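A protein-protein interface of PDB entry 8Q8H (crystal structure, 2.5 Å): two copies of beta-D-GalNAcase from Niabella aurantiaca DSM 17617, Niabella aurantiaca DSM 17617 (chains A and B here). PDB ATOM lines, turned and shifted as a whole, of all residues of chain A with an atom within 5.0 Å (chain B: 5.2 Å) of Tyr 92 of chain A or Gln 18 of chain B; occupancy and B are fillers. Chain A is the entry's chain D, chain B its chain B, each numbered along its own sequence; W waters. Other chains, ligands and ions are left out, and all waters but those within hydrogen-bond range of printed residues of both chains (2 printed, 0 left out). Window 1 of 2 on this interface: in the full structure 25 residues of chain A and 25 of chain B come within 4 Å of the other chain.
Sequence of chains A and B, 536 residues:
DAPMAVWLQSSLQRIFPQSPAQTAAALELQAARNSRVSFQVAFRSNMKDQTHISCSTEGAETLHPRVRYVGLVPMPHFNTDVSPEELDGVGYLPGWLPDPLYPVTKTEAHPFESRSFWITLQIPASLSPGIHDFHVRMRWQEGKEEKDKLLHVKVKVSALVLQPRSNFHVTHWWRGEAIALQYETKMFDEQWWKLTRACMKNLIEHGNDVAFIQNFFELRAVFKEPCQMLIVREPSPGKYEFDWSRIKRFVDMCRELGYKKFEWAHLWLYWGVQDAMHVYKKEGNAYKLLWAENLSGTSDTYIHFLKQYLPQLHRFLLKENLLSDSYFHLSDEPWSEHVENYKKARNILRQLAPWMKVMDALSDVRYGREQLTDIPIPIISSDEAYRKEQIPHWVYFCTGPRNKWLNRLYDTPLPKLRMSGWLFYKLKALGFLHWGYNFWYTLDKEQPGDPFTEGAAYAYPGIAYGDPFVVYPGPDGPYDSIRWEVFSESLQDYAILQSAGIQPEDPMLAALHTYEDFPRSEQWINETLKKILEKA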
ATOM      1  N   PHE A  16      -1.711  -9.744   8.707  1.00  0.00           N
ATOM      2  CA  PHE A  16      -2.543 -10.776   9.294  1.00  0.00           C
ATOM      3  C   PHE A  16      -3.986 -10.566   8.877  1.00  0.00           C
ATOM      4  O   PHE A  16      -4.375  -9.467   8.485  1.00  0.00           O
ATOM      5  CB  PHE A  16      -2.384 -10.783  10.820  1.00  0.00           C
ATOM      6  CG  PHE A  16      -1.010 -11.189  11.254  1.00  0.00           C
ATOM      7  CD1 PHE A  16      -0.685 -12.516  11.422  1.00  0.00           C
ATOM      8  CD2 PHE A  16      -0.010 -10.245  11.386  1.00  0.00           C
ATOM      9  CE1 PHE A  16       0.588 -12.881  11.784  1.00  0.00           C
ATOM     10  CE2 PHE A  16       1.274 -10.611  11.736  1.00  0.00           C
ATOM     11  CZ  PHE A  16       1.570 -11.917  11.926  1.00  0.00           C
ATOM     12  N   GLN A  18      -6.769 -10.105  10.244  1.00  0.00           N
ATOM     13  CA  GLN A  18      -7.537  -9.104  10.962  1.00  0.00           C
ATOM     14  C   GLN A  18      -6.772  -7.791  11.111  1.00  0.00           C
ATOM     15  O   GLN A  18      -7.179  -6.936  11.888  1.00  0.00           O
ATOM     16  CB  GLN A  18      -8.008  -9.711  12.299  1.00  0.00           C
ATOM     17  CG  GLN A  18      -6.955 -10.114  13.349  1.00  0.00           C
ATOM     18  CD  GLN A  18      -6.179 -11.461  13.085  1.00  0.00           C
ATOM     19  OE1 GLN A  18      -5.876 -11.811  11.974  1.00  0.00           O
ATOM     20  NE2 GLN A  18      -5.918 -12.214  14.146  1.00  0.00           N
ATOM     21  N   SER A  19      -5.690  -7.611  10.347  1.00  0.00           N
ATOM     22  CA  SER A  19      -5.035  -6.320  10.192  1.00  0.00           C
ATOM     23  C   SER A  19      -6.013  -5.280   9.645  1.00  0.00           C
ATOM     24  O   SER A  19      -6.844  -5.586   8.782  1.00  0.00           O
ATOM     25  CB  SER A  19      -3.850  -6.406   9.212  1.00  0.00           C
ATOM     26  OG  SER A  19      -2.678  -6.981   9.773  1.00  0.00           O
ATOM     27  N   PRO A  20      -5.900  -4.038  10.070  1.00  0.00           N
ATOM     28  CA  PRO A  20      -6.748  -2.981   9.521  1.00  0.00           C
ATOM     29  C   PRO A  20      -6.280  -2.491   8.169  1.00  0.00           C
ATOM     30  O   PRO A  20      -5.086  -2.513   7.838  1.00  0.00           O
ATOM     31  CB  PRO A  20      -6.644  -1.869  10.565  1.00  0.00           C
ATOM     32  CG  PRO A  20      -5.320  -2.110  11.229  1.00  0.00           C
ATOM     33  CD  PRO A  20      -5.116  -3.587  11.229  1.00  0.00           C
ATOM     34  N   GLY A  89       3.610 -10.600  15.160  1.00  0.00           N
ATOM     35  CA  GLY A  89       2.216 -10.924  15.261  1.00  0.00           C
ATOM     36  C   GLY A  89       1.609 -10.733  16.624  1.00  0.00           C
ATOM     37  O   GLY A  89       0.522 -11.251  16.886  1.00  0.00           O
ATOM     38  N   VAL A  90       2.270 -10.010  17.517  1.00  0.00           N
ATOM     39  CA  VAL A  90       1.618  -9.712  18.779  1.00  0.00           C
ATOM     40  C   VAL A  90       0.343  -8.932  18.503  1.00  0.00           C
ATOM     41  O   VAL A  90       0.360  -7.920  17.794  1.00  0.00           O
ATOM     42  CB  VAL A  90       2.544  -8.932  19.705  1.00  0.00           C
ATOM     43  CG1 VAL A  90       1.758  -8.615  20.945  1.00  0.00           C
ATOM     44  CG2 VAL A  90       3.816  -9.741  20.022  1.00  0.00           C
ATOM     45  N   GLY A  91      -0.762  -9.391  19.083  1.00  0.00           N
ATOM     46  CA  GLY A  91      -2.081  -8.876  18.832  1.00  0.00           C
ATOM     47  C   GLY A  91      -2.858  -9.647  17.793  1.00  0.00           C
ATOM     48  O   GLY A  91      -4.072  -9.455  17.686  1.00  0.00           O
ATOM     49  N   TYR A  92      -2.191 -10.516  17.046  1.00  0.00           N
ATOM     50  CA  TYR A  92      -2.770 -11.270  15.939  1.00  0.00           C
ATOM     51  C   TYR A  92      -2.613 -12.769  16.051  1.00  0.00           C
ATOM     52  O   TYR A  92      -3.388 -13.502  15.453  1.00  0.00           O
ATOM     53  CB  TYR A  92      -2.140 -10.819  14.598  1.00  0.00           C
ATOM     54  CG  TYR A  92      -2.433  -9.375  14.360  1.00  0.00           C
ATOM     55  CD1 TYR A  92      -3.725  -8.962  14.159  1.00  0.00           C
ATOM     56  CD2 TYR A  92      -1.426  -8.415  14.349  1.00  0.00           C
ATOM     57  CE1 TYR A  92      -4.029  -7.666  13.942  1.00  0.00           C
ATOM     58  CE2 TYR A  92      -1.729  -7.080  14.132  1.00  0.00           C
ATOM     59  CZ  TYR A  92      -3.041  -6.726  13.920  1.00  0.00           C
ATOM     60  OH  TYR A  92      -3.433  -5.420  13.701  1.00  0.00           O
ATOM     61  N   LEU A  93      -1.578 -13.223  16.674  1.00  0.00           N
ATOM     62  CA  LEU A  93      -1.342 -14.621  16.857  1.00  0.00           C
ATOM     63  C   LEU A  93      -1.549 -14.995  18.321  1.00  0.00           C
ATOM     64  O   LEU A  93      -1.512 -14.132  19.203  1.00  0.00           O
ATOM     65  CB  LEU A  93       0.091 -14.951  16.423  1.00  0.00           C
ATOM     66  CG  LEU A  93       0.515 -14.801  14.975  1.00  0.00           C
ATOM     67  CD1 LEU A  93       2.000 -15.101  14.864  1.00  0.00           C
ATOM     68  CD2 LEU A  93      -0.293 -15.750  14.137  1.00  0.00           C
ATOM     69  N   PRO A  94      -1.757 -16.279  18.624  1.00  0.00           N
ATOM     70  CA  PRO A  94      -1.940 -17.428  17.745  1.00  0.00           C
ATOM     71  C   PRO A  94      -3.108 -17.211  16.787  1.00  0.00           C
ATOM     72  O   PRO A  94      -4.038 -16.469  17.148  1.00  0.00           O
ATOM     73  CB  PRO A  94      -2.211 -18.584  18.728  1.00  0.00           C
ATOM     74  CG  PRO A  94      -1.553 -18.175  19.987  1.00  0.00           C
ATOM     75  CD  PRO A  94      -1.789 -16.670  20.032  1.00  0.00           C
ATOM     76  N   GLY A  95      -3.040 -17.791  15.589  1.00  0.00           N
ATOM     77  CA  GLY A  95      -4.008 -17.451  14.555  1.00  0.00           C
ATOM     78  C   GLY A  95      -3.501 -17.906  13.195  1.00  0.00           C
ATOM     79  O   GLY A  95      -2.655 -18.784  13.104  1.00  0.00           O
ATOM     80  N   PHE B  16     -10.800 -14.822  22.920  1.00  0.00           N
ATOM     81  CA  PHE B  16      -9.919 -15.251  21.849  1.00  0.00           C
ATOM     82  C   PHE B  16      -8.455 -15.294  22.285  1.00  0.00           C
ATOM     83  O   PHE B  16      -8.025 -14.522  23.160  1.00  0.00           O
ATOM     84  CB  PHE B  16     -10.093 -14.318  20.665  1.00  0.00           C
ATOM     85  CG  PHE B  16     -11.480 -14.360  20.098  1.00  0.00           C
ATOM     86  CD1 PHE B  16     -11.832 -15.371  19.233  1.00  0.00           C
ATOM     87  CD2 PHE B  16     -12.442 -13.420  20.467  1.00  0.00           C
ATOM     88  CE1 PHE B  16     -13.094 -15.456  18.732  1.00  0.00           C
ATOM     89  CE2 PHE B  16     -13.716 -13.498  19.962  1.00  0.00           C
ATOM     90  CZ  PHE B  16     -14.051 -14.502  19.093  1.00  0.00           C
ATOM     91  N   PRO B  17      -7.662 -16.159  21.634  1.00  0.00           N
ATOM     92  CA  PRO B  17      -6.301 -16.418  22.127  1.00  0.00           C
ATOM     93  C   PRO B  17      -5.487 -15.158  22.318  1.00  0.00           C
ATOM     94  O   PRO B  17      -4.633 -15.080  23.213  1.00  0.00           O
ATOM     95  CB  PRO B  17      -5.678 -17.273  21.018  1.00  0.00           C
ATOM     96  CG  PRO B  17      -6.848 -17.801  20.237  1.00  0.00           C
ATOM     97  CD  PRO B  17      -7.915 -16.796  20.337  1.00  0.00           C
ATOM     98  N   GLN B  18      -5.705 -14.175  21.460  1.00  0.00           N
ATOM     99  CA  GLN B  18      -4.924 -12.957  21.467  1.00  0.00           C
ATOM    100  C   GLN B  18      -5.665 -11.821  22.175  1.00  0.00           C
ATOM    101  O   GLN B  18      -5.220 -10.671  22.145  1.00  0.00           O
ATOM    102  CB  GLN B  18      -4.524 -12.652  20.024  1.00  0.00           C
ATOM    103  CG  GLN B  18      -5.612 -12.171  19.044  1.00  0.00           C
ATOM    104  CD  GLN B  18      -6.484 -13.262  18.384  1.00  0.00           C
ATOM    105  OE1 GLN B  18      -6.764 -14.304  18.955  1.00  0.00           O
ATOM    106  NE2 GLN B  18      -6.883 -13.010  17.154  1.00  0.00           N
ATOM    107  N   SER B  19      -6.735 -12.162  22.888  1.00  0.00           N
ATOM    108  CA  SER B  19      -7.388 -11.256  23.802  1.00  0.00           C
ATOM    109  C   SER B  19      -6.369 -10.805  24.839  1.00  0.00           C
ATOM    110  O   SER B  19      -5.417 -11.537  25.130  1.00  0.00           O
ATOM    111  CB  SER B  19      -8.552 -11.933  24.537  1.00  0.00           C
ATOM    112  OG  SER B  19      -9.708 -12.150  23.725  1.00  0.00           O
ATOM    113  N   PRO B  20      -6.519  -9.594  25.362  1.00  0.00           N
ATOM    114  CA  PRO B  20      -5.686  -9.140  26.475  1.00  0.00           C
ATOM    115  C   PRO B  20      -6.169  -9.686  27.809  1.00  0.00           C
ATOM    116  O   PRO B  20      -7.360  -9.951  28.005  1.00  0.00           O
ATOM    117  CB  PRO B  20      -5.851  -7.616  26.427  1.00  0.00           C
ATOM    118  CG  PRO B  20      -7.265  -7.446  25.904  1.00  0.00           C
ATOM    119  CD  PRO B  20      -7.482  -8.571  24.923  1.00  0.00           C
ATOM    120  N   GLY B  91     -11.951  -7.998  14.915  1.00  0.00           N
ATOM    121  CA  GLY B  91     -10.623  -7.753  15.436  1.00  0.00           C
ATOM    122  C   GLY B  91      -9.862  -8.990  15.845  1.00  0.00           C
ATOM    123  O   GLY B  91      -8.661  -8.899  16.102  1.00  0.00           O
ATOM    124  N   TYR B  92     -10.519 -10.138  15.939  1.00  0.00           N
ATOM    125  CA  TYR B  92      -9.860 -11.366  16.355  1.00  0.00           C
ATOM    126  C   TYR B  92      -9.982 -12.499  15.351  1.00  0.00           C
ATOM    127  O   TYR B  92      -9.084 -13.332  15.285  1.00  0.00           O
ATOM    128  CB  TYR B  92     -10.416 -11.848  17.709  1.00  0.00           C
ATOM    129  CG  TYR B  92     -10.218 -10.841  18.805  1.00  0.00           C
ATOM    130  CD1 TYR B  92      -8.962 -10.582  19.313  1.00  0.00           C
ATOM    131  CD2 TYR B  92     -11.292 -10.149  19.339  1.00  0.00           C
ATOM    132  CE1 TYR B  92      -8.775  -9.670  20.332  1.00  0.00           C
ATOM    133  CE2 TYR B  92     -11.118  -9.220  20.343  1.00  0.00           C
ATOM    134  CZ  TYR B  92      -9.862  -8.994  20.851  1.00  0.00           C
ATOM    135  OH  TYR B  92      -9.675  -8.082  21.875  1.00  0.00           O
ATOM    136  N   LEU B  93     -11.049 -12.558  14.592  1.00  0.00           N
ATOM    137  CA  LEU B  93     -11.245 -13.533  13.536  1.00  0.00           C
ATOM    138  C   LEU B  93     -10.997 -12.863  12.184  1.00  0.00           C
ATOM    139  O   LEU B  93     -10.986 -11.634  12.091  1.00  0.00           O
ATOM    140  CB  LEU B  93     -12.673 -14.075  13.578  1.00  0.00           C
ATOM    141  CG  LEU B  93     -13.065 -14.809  14.851  1.00  0.00           C
ATOM    142  CD1 LEU B  93     -14.596 -15.114  14.846  1.00  0.00           C
ATOM    143  CD2 LEU B  93     -12.199 -16.052  14.985  1.00  0.00           C
ATOM    144  N   PHE B 112       1.507 -16.334  26.132  1.00  0.00           N
ATOM    145  CA  PHE B 112       0.849 -15.135  25.630  1.00  0.00           C
ATOM    146  C   PHE B 112      -0.459 -15.486  24.962  1.00  0.00           C
ATOM    147  O   PHE B 112      -0.846 -14.864  23.972  1.00  0.00           O
ATOM    148  CB  PHE B 112       1.778 -14.342  24.695  1.00  0.00           C
ATOM    149  CG  PHE B 112       3.157 -14.143  25.303  1.00  0.00           C
ATOM    150  CD1 PHE B 112       3.301 -13.440  26.493  1.00  0.00           C
ATOM    151  CD2 PHE B 112       4.267 -14.702  24.739  1.00  0.00           C
ATOM    152  CE1 PHE B 112       4.515 -13.326  27.115  1.00  0.00           C
ATOM    153  CE2 PHE B 112       5.508 -14.556  25.343  1.00  0.00           C
ATOM    154  CZ  PHE B 112       5.628 -13.885  26.536  1.00  0.00           C
ATOM    155  N   SER B 114      -4.509 -16.351  25.733  1.00  0.00           N
ATOM    156  CA  SER B 114      -5.647 -16.313  26.641  1.00  0.00           C
ATOM    157  C   SER B 114      -6.573 -17.485  26.342  1.00  0.00           C
ATOM    158  O   SER B 114      -7.027 -17.647  25.204  1.00  0.00           O
ATOM    159  CB  SER B 114      -6.429 -15.014  26.495  1.00  0.00           C
ATOM    160  OG  SER B 114      -5.748 -13.881  26.985  1.00  0.00           O
HETATM  161  O   HOH W   1      -6.191 -10.322  16.390  1.00  0.00           O
HETATM  162  O   HOH W   2      -6.790 -16.661  16.709  1.00  0.00           O
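Gln 18 of chain A touches its own counterpart, Gln 18 of chain B.
Gln 18 of chain A touches Gly 91 of chain B, and with the chains exchanged Gly 91 of chain A touches Gln 18 of chain B.
Gln 18 of chain A touches Tyr 92 of chain B, and with the chains exchanged Tyr 92 of chain A touches Gln 18 of chain B.
Gln 18 of chain A touches Leu 93 of chain B, and with the chains exchanged Leu 93 of chain A touches Gln 18 of chain B.
Of the 8 pairs that touch across the chains among the printed residues, 7 have their exchanged pair printed and touching as well.
Water W1 lies within hydrogen-bond range of the backbone carbonyl oxygen of Gly 91 of chain A, the backbone carbonyl oxygen of Gly 91 of chain B, the side-chain amide nitrogen of Gln 18 of chain B and the side-chain amide nitrogen of Gln 18 of chain A.
Water W2 bridges O of Pro 94 of chain A and OE1 of Gln 18 of chain B.
The side-chain amide nitrogen (NE2) of Gln 18 of chain A sits close to the side-chain amide nitrogen (NE2) of Gln 18 of chain B (3.3 Å).
Along chain A the printed residues that touch a printed residue of chain B span positions 18 to 94.
Of the 10 printed residues of chain B, 4 touch a printed residue of chain A.
Printed residues of chain B that touch a printed residue of chain A: Gln 18, Gly 91, Tyr 92 and Leu 93.
Among the printed residues, 8 pairs touch across the chains.
Among the printed residues, no Asp or Glu carboxylate lies within 4 Å of a Lys or Arg side-chain nitrogen of the other chain.
Of chain B, only Gln 18 comes within 4 Å of Tyr 92 of chain A.
Gln 18 of chain B touches just these residues of chain A: Gln 18, Gly 91, Tyr 92, Leu 93 and Pro 94.
Of the printed residues of chain A, Gly 91 of chain B touches Gln 18 (3.5 Å).
Of the printed residues of chain B, Leu 93 of chain A touches Gln 18 (3.5 Å).
Printed residues of chain A within 4 Å of Tyr 92 of chain B: Gln 18.
Printed residues of chain B within 4 Å of Gly 91 of chain A: Gln 18 (3.4 Å).
Of the printed residues of chain B, Pro 94 of chain A touches Gln 18.
Pro 17 of chain B touches none of the printed residues of chain A.
Ser 19 of chain B touches none of the printed residues of chain A.
The nearest printed residue of chain B that does not touch Tyr 92 of chain A is Gly 91 of chain B (5.3 Å).
The nearest printed residue of chain A that does not touch Gln 18 of chain B is Gly 95 of chain A (5.9 Å).
NE2 of Gln 18 of chain B sits at hydrogen-bond distance from O of Tyr 92 of chain B, at 2.9 Å.
The side-chain amide nitrogen (NE2) of Gln 18 of chain A sits at hydrogen-bond distance from the backbone carbonyl oxygen (O) of Tyr 92 of chain A (3.1 Å).
CG of Gln 18 of chain A touches O of Gly 91 of chain B, at 3.5 Å.
Gln 18 of chain A touches Tyr 92 of chain B.
O of Leu 93 of chain B touches CB of Gln 18 of chain A (3.6 Å).
Gln 18 of chain B touches Gly 91 of chain A (CG to O, 3.4 Å).
Gln 18 of chain B touches Tyr 92 of chain A.
Gln 18 of chain B touches Leu 93 of chain A (CB to O, 3.5 Å).
Pro 94 of chain A touches Gln 18 of chain B (O to OE1, 3.9 Å).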
